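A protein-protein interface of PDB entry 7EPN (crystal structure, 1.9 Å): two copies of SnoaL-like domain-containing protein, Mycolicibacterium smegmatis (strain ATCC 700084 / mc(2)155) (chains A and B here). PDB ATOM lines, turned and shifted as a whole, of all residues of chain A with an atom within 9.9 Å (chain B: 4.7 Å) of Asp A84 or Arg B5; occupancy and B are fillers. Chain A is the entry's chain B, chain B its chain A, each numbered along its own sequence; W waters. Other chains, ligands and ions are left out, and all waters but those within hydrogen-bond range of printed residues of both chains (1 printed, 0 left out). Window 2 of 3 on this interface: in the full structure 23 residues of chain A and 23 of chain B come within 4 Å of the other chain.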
ATOM      1  N   SER A   3     -21.501  41.404 -27.589  1.00  0.00           N
ATOM      2  CA  SER A   3     -20.742  40.343 -26.940  1.00  0.00           C
ATOM      3  C   SER A   3     -21.586  39.082 -26.770  1.00  0.00           C
ATOM      4  O   SER A   3     -22.820  39.115 -26.733  1.00  0.00           O
ATOM      5  CB  SER A   3     -20.236  40.801 -25.578  1.00  0.00           C
ATOM      6  OG  SER A   3     -21.310  40.852 -24.650  1.00  0.00           O
ATOM      7  N   THR A   4     -20.896  37.949 -26.660  1.00  0.00           N
ATOM      8  CA  THR A   4     -21.589  36.698 -26.356  1.00  0.00           C
ATOM      9  C   THR A   4     -22.412  36.833 -25.086  1.00  0.00           C
ATOM     10  O   THR A   4     -23.583  36.439 -25.049  1.00  0.00           O
ATOM     11  CB  THR A   4     -20.580  35.560 -26.208  1.00  0.00           C
ATOM     12  OG1 THR A   4     -19.856  35.419 -27.428  1.00  0.00           O
ATOM     13  CG2 THR A   4     -21.279  34.234 -25.878  1.00  0.00           C
ATOM     14  N   ARG A   5     -21.822  37.424 -24.041  1.00  0.00           N
ATOM     15  CA  ARG A   5     -22.529  37.522 -22.765  1.00  0.00           C
ATOM     16  C   ARG A   5     -23.820  38.316 -22.902  1.00  0.00           C
ATOM     17  O   ARG A   5     -24.852  37.939 -22.327  1.00  0.00           O
ATOM     18  CB  ARG A   5     -21.635  38.155 -21.700  1.00  0.00           C
ATOM     19  CG  ARG A   5     -22.163  37.976 -20.273  1.00  0.00           C
ATOM     20  CD  ARG A   5     -21.102  38.420 -19.248  1.00  0.00           C
ATOM     21  NE  ARG A   5     -20.110  37.369 -18.992  1.00  0.00           N
ATOM     22  CZ  ARG A   5     -20.325  36.344 -18.179  1.00  0.00           C
ATOM     23  NH1 ARG A   5     -21.495  36.241 -17.545  1.00  0.00           N
ATOM     24  NH2 ARG A   5     -19.377  35.432 -17.995  1.00  0.00           N
ATOM     25  N   VAL A   8     -26.432  36.187 -24.627  1.00  0.00           N
ATOM     26  CA  VAL A   8     -26.933  35.157 -23.721  1.00  0.00           C
ATOM     27  C   VAL A   8     -27.871  35.762 -22.681  1.00  0.00           C
ATOM     28  O   VAL A   8     -28.924  35.180 -22.361  1.00  0.00           O
ATOM     29  CB  VAL A   8     -25.750  34.412 -23.076  1.00  0.00           C
ATOM     30  CG1 VAL A   8     -26.238  33.432 -21.985  1.00  0.00           C
ATOM     31  CG2 VAL A   8     -24.940  33.684 -24.176  1.00  0.00           C
ATOM     32  N   VAL A  81     -23.122  32.056 -15.304  1.00  0.00           N
ATOM     33  CA  VAL A  81     -23.028  32.078 -16.758  1.00  0.00           C
ATOM     34  C   VAL A  81     -21.543  32.133 -17.097  1.00  0.00           C
ATOM     35  O   VAL A  81     -20.878  33.140 -16.813  1.00  0.00           O
ATOM     36  CB  VAL A  81     -23.771  33.272 -17.366  1.00  0.00           C
ATOM     37  CG1 VAL A  81     -23.495  33.345 -18.844  1.00  0.00           C
ATOM     38  CG2 VAL A  81     -25.276  33.179 -17.087  1.00  0.00           C
ATOM     39  N   LEU A  82     -21.010  31.054 -17.661  1.00  0.00           N
ATOM     40  CA  LEU A  82     -19.612  31.020 -18.094  1.00  0.00           C
ATOM     41  C   LEU A  82     -19.549  31.354 -19.573  1.00  0.00           C
ATOM     42  O   LEU A  82     -20.388  30.899 -20.344  1.00  0.00           O
ATOM     43  CB  LEU A  82     -18.957  29.654 -17.876  1.00  0.00           C
ATOM     44  CG  LEU A  82     -18.885  29.121 -16.447  1.00  0.00           C
ATOM     45  CD1 LEU A  82     -18.604  30.234 -15.418  1.00  0.00           C
ATOM     46  CD2 LEU A  82     -20.160  28.413 -16.146  1.00  0.00           C
ATOM     47  N   VAL A  83     -18.572  32.171 -19.954  1.00  0.00           N
ATOM     48  CA  VAL A  83     -18.431  32.638 -21.332  1.00  0.00           C
ATOM     49  C   VAL A  83     -16.987  32.434 -21.760  1.00  0.00           C
ATOM     50  O   VAL A  83     -16.055  32.816 -21.040  1.00  0.00           O
ATOM     51  CB  VAL A  83     -18.830  34.122 -21.496  1.00  0.00           C
ATOM     52  CG1 VAL A  83     -18.604  34.579 -22.949  1.00  0.00           C
ATOM     53  CG2 VAL A  83     -20.299  34.331 -21.101  1.00  0.00           C
ATOM     54  N   ASP A  84     -16.805  31.863 -22.944  1.00  0.00           N
ATOM     55  CA  ASP A  84     -15.475  31.600 -23.481  1.00  0.00           C
ATOM     56  C   ASP A  84     -15.602  31.774 -24.994  1.00  0.00           C
ATOM     57  O   ASP A  84     -16.089  30.871 -25.681  1.00  0.00           O
ATOM     58  CB  ASP A  84     -15.005  30.201 -23.090  1.00  0.00           C
ATOM     59  CG  ASP A  84     -13.601  29.860 -23.619  1.00  0.00           C
ATOM     60  OD1 ASP A  84     -12.947  30.736 -24.231  1.00  0.00           O
ATOM     61  OD2 ASP A  84     -13.148  28.701 -23.402  1.00  0.00           O
ATOM     62  N   GLY A  85     -15.191  32.942 -25.494  1.00  0.00           N
ATOM     63  CA  GLY A  85     -15.300  33.203 -26.923  1.00  0.00           C
ATOM     64  C   GLY A  85     -16.755  33.279 -27.340  1.00  0.00           C
ATOM     65  O   GLY A  85     -17.560  33.987 -26.726  1.00  0.00           O
ATOM     66  N   ALA A  86     -17.104  32.551 -28.398  1.00  0.00           N
ATOM     67  CA  ALA A  86     -18.474  32.529 -28.900  1.00  0.00           C
ATOM     68  C   ALA A  86     -19.374  31.568 -28.138  1.00  0.00           C
ATOM     69  O   ALA A  86     -20.571  31.478 -28.449  1.00  0.00           O
ATOM     70  CB  ALA A  86     -18.481  32.152 -30.380  1.00  0.00           C
ATOM     71  N   ASP A  87     -18.831  30.830 -27.178  1.00  0.00           N
ATOM     72  CA  ASP A  87     -19.598  29.844 -26.440  1.00  0.00           C
ATOM     73  C   ASP A  87     -19.893  30.332 -25.029  1.00  0.00           C
ATOM     74  O   ASP A  87     -19.176  31.158 -24.452  1.00  0.00           O
ATOM     75  CB  ASP A  87     -18.863  28.504 -26.363  1.00  0.00           C
ATOM     76  CG  ASP A  87     -18.663  27.869 -27.732  1.00  0.00           C
ATOM     77  OD1 ASP A  87     -17.724  28.284 -28.444  1.00  0.00           O
ATOM     78  OD2 ASP A  87     -19.441  26.959 -28.084  1.00  0.00           O
ATOM     79  N   ALA A  88     -20.963  29.788 -24.476  1.00  0.00           N
ATOM     80  CA  ALA A  88     -21.321  30.052 -23.095  1.00  0.00           C
ATOM     81  C   ALA A  88     -22.013  28.825 -22.544  1.00  0.00           C
ATOM     82  O   ALA A  88     -22.617  28.051 -23.291  1.00  0.00           O
ATOM     83  CB  ALA A  88     -22.232  31.281 -22.953  1.00  0.00           C
ATOM     84  N   VAL A  89     -21.951  28.668 -21.224  1.00  0.00           N
ATOM     85  CA  VAL A  89     -22.712  27.629 -20.541  1.00  0.00           C
ATOM     86  C   VAL A  89     -23.447  28.293 -19.388  1.00  0.00           C
ATOM     87  O   VAL A  89     -22.831  28.988 -18.571  1.00  0.00           O
ATOM     88  CB  VAL A  89     -21.832  26.472 -20.032  1.00  0.00           C
ATOM     89  CG1 VAL A  89     -22.704  25.461 -19.293  1.00  0.00           C
ATOM     90  CG2 VAL A  89     -21.134  25.774 -21.196  1.00  0.00           C
ATOM     91  N   VAL A  90     -24.763  28.118 -19.352  1.00  0.00           N
ATOM     92  CA  VAL A  90     -25.603  28.657 -18.289  1.00  0.00           C
ATOM     93  C   VAL A  90     -25.856  27.524 -17.303  1.00  0.00           C
ATOM     94  O   VAL A  90     -26.338  26.456 -17.697  1.00  0.00           O
ATOM     95  CB  VAL A  90     -26.919  29.220 -18.850  1.00  0.00           C
ATOM     96  CG1 VAL A  90     -27.844  29.683 -17.703  1.00  0.00           C
ATOM     97  CG2 VAL A  90     -26.648  30.371 -19.832  1.00  0.00           C
ATOM     98  N   HIS A 112     -25.624  24.865 -22.947  1.00  0.00           N
ATOM     99  CA  HIS A 112     -24.457  25.266 -23.725  1.00  0.00           C
ATOM    100  C   HIS A 112     -24.943  25.983 -24.978  1.00  0.00           C
ATOM    101  O   HIS A 112     -25.698  25.409 -25.766  1.00  0.00           O
ATOM    102  CB  HIS A 112     -23.614  24.037 -24.084  1.00  0.00           C
ATOM    103  CG  HIS A 112     -22.488  24.327 -25.031  1.00  0.00           C
ATOM    104  ND1 HIS A 112     -22.090  23.446 -26.015  1.00  0.00           N
ATOM    105  CD2 HIS A 112     -21.672  25.402 -25.138  1.00  0.00           C
ATOM    106  CE1 HIS A 112     -21.077  23.965 -26.689  1.00  0.00           C
ATOM    107  NE2 HIS A 112     -20.798  25.150 -26.171  1.00  0.00           N
ATOM    108  N   LEU A 113     -24.519  27.232 -25.156  1.00  0.00           N
ATOM    109  CA  LEU A 113     -24.941  28.059 -26.274  1.00  0.00           C
ATOM    110  C   LEU A 113     -23.739  28.437 -27.126  1.00  0.00           C
ATOM    111  O   LEU A 113     -22.623  28.569 -26.624  1.00  0.00           O
ATOM    112  CB  LEU A 113     -25.648  29.345 -25.781  1.00  0.00           C
ATOM    113  CG  LEU A 113     -26.870  29.047 -24.907  1.00  0.00           C
ATOM    114  CD1 LEU A 113     -27.248  30.225 -23.993  1.00  0.00           C
ATOM    115  CD2 LEU A 113     -28.024  28.648 -25.833  1.00  0.00           C
ATOM    116  N   THR A 114     -23.975  28.613 -28.424  1.00  0.00           N
ATOM    117  CA  THR A 114     -22.986  29.233 -29.296  1.00  0.00           C
ATOM    118  C   THR A 114     -23.677  30.367 -30.034  1.00  0.00           C
ATOM    119  O   THR A 114     -24.835  30.231 -30.437  1.00  0.00           O
ATOM    120  CB  THR A 114     -22.371  28.236 -30.294  1.00  0.00           C
ATOM    121  OG1 THR A 114     -21.825  27.117 -29.578  1.00  0.00           O
ATOM    122  CG2 THR A 114     -21.250  28.920 -31.103  1.00  0.00           C
ATOM    123  N   VAL A 115     -22.989  31.498 -30.175  1.00  0.00           N
ATOM    124  CA  VAL A 115     -23.563  32.660 -30.836  1.00  0.00           C
ATOM    125  C   VAL A 115     -22.664  33.060 -31.993  1.00  0.00           C
ATOM    126  O   VAL A 115     -21.434  33.012 -31.881  1.00  0.00           O
ATOM    127  CB  VAL A 115     -23.766  33.849 -29.870  1.00  0.00           C
ATOM    128  CG1 VAL A 115     -24.702  33.471 -28.743  1.00  0.00           C
ATOM    129  CG2 VAL A 115     -22.451  34.363 -29.331  1.00  0.00           C
ATOM    130  N   GLU A 116     -23.285  33.439 -33.108  1.00  0.00           N
ATOM    131  CA  GLU A 116     -22.584  33.963 -34.272  1.00  0.00           C
ATOM    132  C   GLU A 116     -23.427  35.089 -34.836  1.00  0.00           C
ATOM    133  O   GLU A 116     -24.626  34.904 -35.061  1.00  0.00           O
ATOM    134  CB  GLU A 116     -22.355  32.888 -35.354  1.00  0.00           C
ATOM    135  CG  GLU A 116     -21.797  31.556 -34.838  1.00  0.00           C
ATOM    136  CD  GLU A 116     -20.363  31.640 -34.310  1.00  0.00           C
ATOM    137  OE1 GLU A 116     -19.785  32.750 -34.270  1.00  0.00           O
ATOM    138  OE2 GLU A 116     -19.817  30.592 -33.898  1.00  0.00           O
ATOM    139  N   SER B   3      -2.652  27.194 -14.608  1.00  0.00           N
ATOM    140  CA  SER B   3      -3.936  27.778 -14.950  1.00  0.00           C
ATOM    141  C   SER B   3      -5.075  26.789 -14.697  1.00  0.00           C
ATOM    142  O   SER B   3      -4.870  25.586 -14.510  1.00  0.00           O
ATOM    143  CB  SER B   3      -3.937  28.216 -16.411  1.00  0.00           C
ATOM    144  OG  SER B   3      -3.974  27.079 -17.256  1.00  0.00           O
ATOM    145  N   THR B   4      -6.299  27.326 -14.712  1.00  0.00           N
ATOM    146  CA  THR B   4      -7.493  26.486 -14.662  1.00  0.00           C
ATOM    147  C   THR B   4      -7.487  25.474 -15.800  1.00  0.00           C
ATOM    148  O   THR B   4      -7.711  24.277 -15.585  1.00  0.00           O
ATOM    149  CB  THR B   4      -8.749  27.359 -14.734  1.00  0.00           C
ATOM    150  OG1 THR B   4      -8.769  28.275 -13.636  1.00  0.00           O
ATOM    151  CG2 THR B   4     -10.026  26.507 -14.701  1.00  0.00           C
ATOM    152  N   ARG B   5      -7.217  25.939 -17.028  1.00  0.00           N
ATOM    153  CA  ARG B   5      -7.266  25.030 -18.168  1.00  0.00           C
ATOM    154  C   ARG B   5      -6.185  23.963 -18.067  1.00  0.00           C
ATOM    155  O   ARG B   5      -6.420  22.803 -18.427  1.00  0.00           O
ATOM    156  CB  ARG B   5      -7.135  25.804 -19.481  1.00  0.00           C
ATOM    157  CG  ARG B   5      -7.375  24.922 -20.696  1.00  0.00           C
ATOM    158  CD  ARG B   5      -7.323  25.710 -21.977  1.00  0.00           C
ATOM    159  NE  ARG B   5      -8.423  26.671 -22.097  1.00  0.00           N
ATOM    160  CZ  ARG B   5      -9.629  26.362 -22.552  1.00  0.00           C
ATOM    161  NH1 ARG B   5      -9.901  25.108 -22.900  1.00  0.00           N
ATOM    162  NH2 ARG B   5     -10.558  27.301 -22.658  1.00  0.00           N
ATOM    163  N   GLU B   6      -4.995  24.332 -17.584  1.00  0.00           N
ATOM    164  CA  GLU B   6      -3.947  23.334 -17.405  1.00  0.00           C
ATOM    165  C   GLU B   6      -4.377  22.275 -16.408  1.00  0.00           C
ATOM    166  O   GLU B   6      -4.110  21.083 -16.601  1.00  0.00           O
ATOM    167  CB  GLU B   6      -2.648  24.002 -16.940  1.00  0.00           C
ATOM    168  CG  GLU B   6      -1.974  24.871 -17.990  1.00  0.00           C
ATOM    169  CD  GLU B   6      -1.943  24.219 -19.363  1.00  0.00           C
ATOM    170  OE1 GLU B   6      -1.327  23.137 -19.494  1.00  0.00           O
ATOM    171  OE2 GLU B   6      -2.534  24.786 -20.311  1.00  0.00           O
ATOM    172  N   THR B   7      -5.045  22.694 -15.326  1.00  0.00           N
ATOM    173  CA  THR B   7      -5.514  21.730 -14.338  1.00  0.00           C
ATOM    174  C   THR B   7      -6.580  20.821 -14.936  1.00  0.00           C
ATOM    175  O   THR B   7      -6.551  19.600 -14.739  1.00  0.00           O
ATOM    176  CB  THR B   7      -6.040  22.472 -13.104  1.00  0.00           C
ATOM    177  OG1 THR B   7      -4.956  23.169 -12.471  1.00  0.00           O
ATOM    178  CG2 THR B   7      -6.686  21.508 -12.103  1.00  0.00           C
ATOM    179  N   VAL B   8      -7.511  21.399 -15.693  1.00  0.00           N
ATOM    180  CA  VAL B   8      -8.564  20.608 -16.327  1.00  0.00           C
ATOM    181  C   VAL B   8      -7.973  19.650 -17.355  1.00  0.00           C
ATOM    182  O   VAL B   8      -8.358  18.475 -17.427  1.00  0.00           O
ATOM    183  CB  VAL B   8      -9.617  21.553 -16.939  1.00  0.00           C
ATOM    184  CG1 VAL B   8     -10.662  20.773 -17.749  1.00  0.00           C
ATOM    185  CG2 VAL B   8     -10.267  22.377 -15.831  1.00  0.00           C
ATOM    186  N   ASN B   9      -7.011  20.124 -18.154  1.00  0.00           N
ATOM    187  CA  ASN B   9      -6.397  19.243 -19.146  1.00  0.00           C
ATOM    188  C   ASN B   9      -5.671  18.080 -18.476  1.00  0.00           C
ATOM    189  O   ASN B   9      -5.692  16.955 -18.985  1.00  0.00           O
ATOM    190  CB  ASN B   9      -5.444  20.034 -20.038  1.00  0.00           C
ATOM    191  CG  ASN B   9      -6.177  20.925 -21.027  1.00  0.00           C
ATOM    192  OD1 ASN B   9      -7.377  20.768 -21.250  1.00  0.00           O
ATOM    193  ND2 ASN B   9      -5.453  21.865 -21.623  1.00  0.00           N
ATOM    194  N   VAL B  81     -13.873  22.101 -24.243  1.00  0.00           N
ATOM    195  CA  VAL B  81     -13.505  22.505 -22.891  1.00  0.00           C
ATOM    196  C   VAL B  81     -13.621  24.019 -22.832  1.00  0.00           C
ATOM    197  O   VAL B  81     -12.802  24.737 -23.425  1.00  0.00           O
ATOM    198  CB  VAL B  81     -12.090  22.053 -22.504  1.00  0.00           C
ATOM    199  CG1 VAL B  81     -11.747  22.578 -21.119  1.00  0.00           C
ATOM    200  CG2 VAL B  81     -11.992  20.550 -22.520  1.00  0.00           C
ATOM    201  N   LEU B  82     -14.622  24.508 -22.114  1.00  0.00           N
ATOM    202  CA  LEU B  82     -14.787  25.939 -21.929  1.00  0.00           C
ATOM    203  C   LEU B  82     -14.210  26.334 -20.581  1.00  0.00           C
ATOM    204  O   LEU B  82     -14.423  25.641 -19.583  1.00  0.00           O
ATOM    205  CB  LEU B  82     -16.256  26.340 -22.007  1.00  0.00           C
ATOM    206  CG  LEU B  82     -16.906  25.844 -23.306  1.00  0.00           C
ATOM    207  CD1 LEU B  82     -18.346  26.312 -23.402  1.00  0.00           C
ATOM    208  CD2 LEU B  82     -16.103  26.287 -24.530  1.00  0.00           C
ATOM    209  N   VAL B  83     -13.472  27.443 -20.555  1.00  0.00           N
ATOM    210  CA  VAL B  83     -12.835  27.925 -19.331  1.00  0.00           C
ATOM    211  C   VAL B  83     -13.137  29.406 -19.198  1.00  0.00           C
ATOM    212  O   VAL B  83     -13.001  30.160 -20.169  1.00  0.00           O
ATOM    213  CB  VAL B  83     -11.308  27.690 -19.330  1.00  0.00           C
ATOM    214  CG1 VAL B  83     -10.665  28.241 -18.056  1.00  0.00           C
ATOM    215  CG2 VAL B  83     -10.977  26.199 -19.504  1.00  0.00           C
HETATM  216  O   HOH W   1     -13.229  32.801 -20.842  1.00  0.00           O
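Hydrophobic or aromatic side chains of chain B within 4 Å of the printed part of chain A: Leu B82.
Of the 19 printed residues of chain A, 4 touch a printed residue of chain B.
Hydrophobic or aromatic side chains of chain A within 4 Å of the printed part of chain B: Val A89 and His A112.
Among the printed residues, Asp or Glu carboxylates within 4 Å of a Lys or Arg side-chain nitrogen of the other chain: Asp A84 with Arg B5 (3.0 Å).
The side-chain hydroxyl (OG) of Ser B3 lies close to the backbone NH (N) of Arg B5 (3.4 Å).
The backbone carbonyl oxygen (O) of Arg B5 sits close to the side-chain amide nitrogen (ND2) of Asn B9.
The guanidinium group (NH1) of Arg B5 lies within hydrogen-bond range of the backbone carbonyl oxygen (O) of Val B81.
N of Val A89 is in hydrogen-bond range of O of Leu A82.
The side-chain carboxylate (OD2) of Asp A87 is in hydrogen-bond range of a ring nitrogen (NE2) of His A112 (3.0 Å).
The side-chain carboxylate (OD2) of Asp A87 is in hydrogen-bond range of the side-chain hydroxyl (OG1) of Thr A114, 2.8 Å away.
The guanidinium group (NH2) of Arg B5 is in salt-bridge range of the side-chain carboxylate (OD2) of Asp A84.
OD2 of Asp A84 is in hydrogen-bond range of N of Val B83, at 3.1 Å.
Water W1 bridges the backbone carbonyl oxygen of Val B83 (2.7 Å) and the backbone carbonyl oxygen of Val A83 (2.8 Å).
Positions printed for both chains: 3, 4, 5, 8, 81, 82 and 83.
Printed residues of chain B within 4 Å of Asp A84: Arg B5 (3.0 Å), Val B81 (3.98 Å), Leu B82 (3.5 Å) and Val B83 (3.1 Å).
Of the printed residues of chain B, Asp A87 touches Leu B82 (3.7 Å).
Printed residues of chain B within 4 Å of Val A89: Leu B82.
Of the printed residues of chain B, His A112 touches Leu B82 (3.9 Å).
Arg B5 touches just one residue of chain A: Asp A84 (3.0 Å).
No residue of chain A comes within 4 Å of Glu B6.
No residue of chain A comes within 4 Å of Val B8.
Val B81 touches just one residue of chain A: Asp A84 (3.98 Å).
Val B83 touches just one residue of chain A: Asp A84.
Among the printed residues, merely in contact across the chains: Asp A84 with Val B81 (3.98 Å), Asp A84 with Leu B82 (3.5 Å), Asp A87 with Leu B82 (3.7 Å), Val A89 with Leu B82 (3.6 Å) and His A112 with Leu B82 (3.9 Å).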
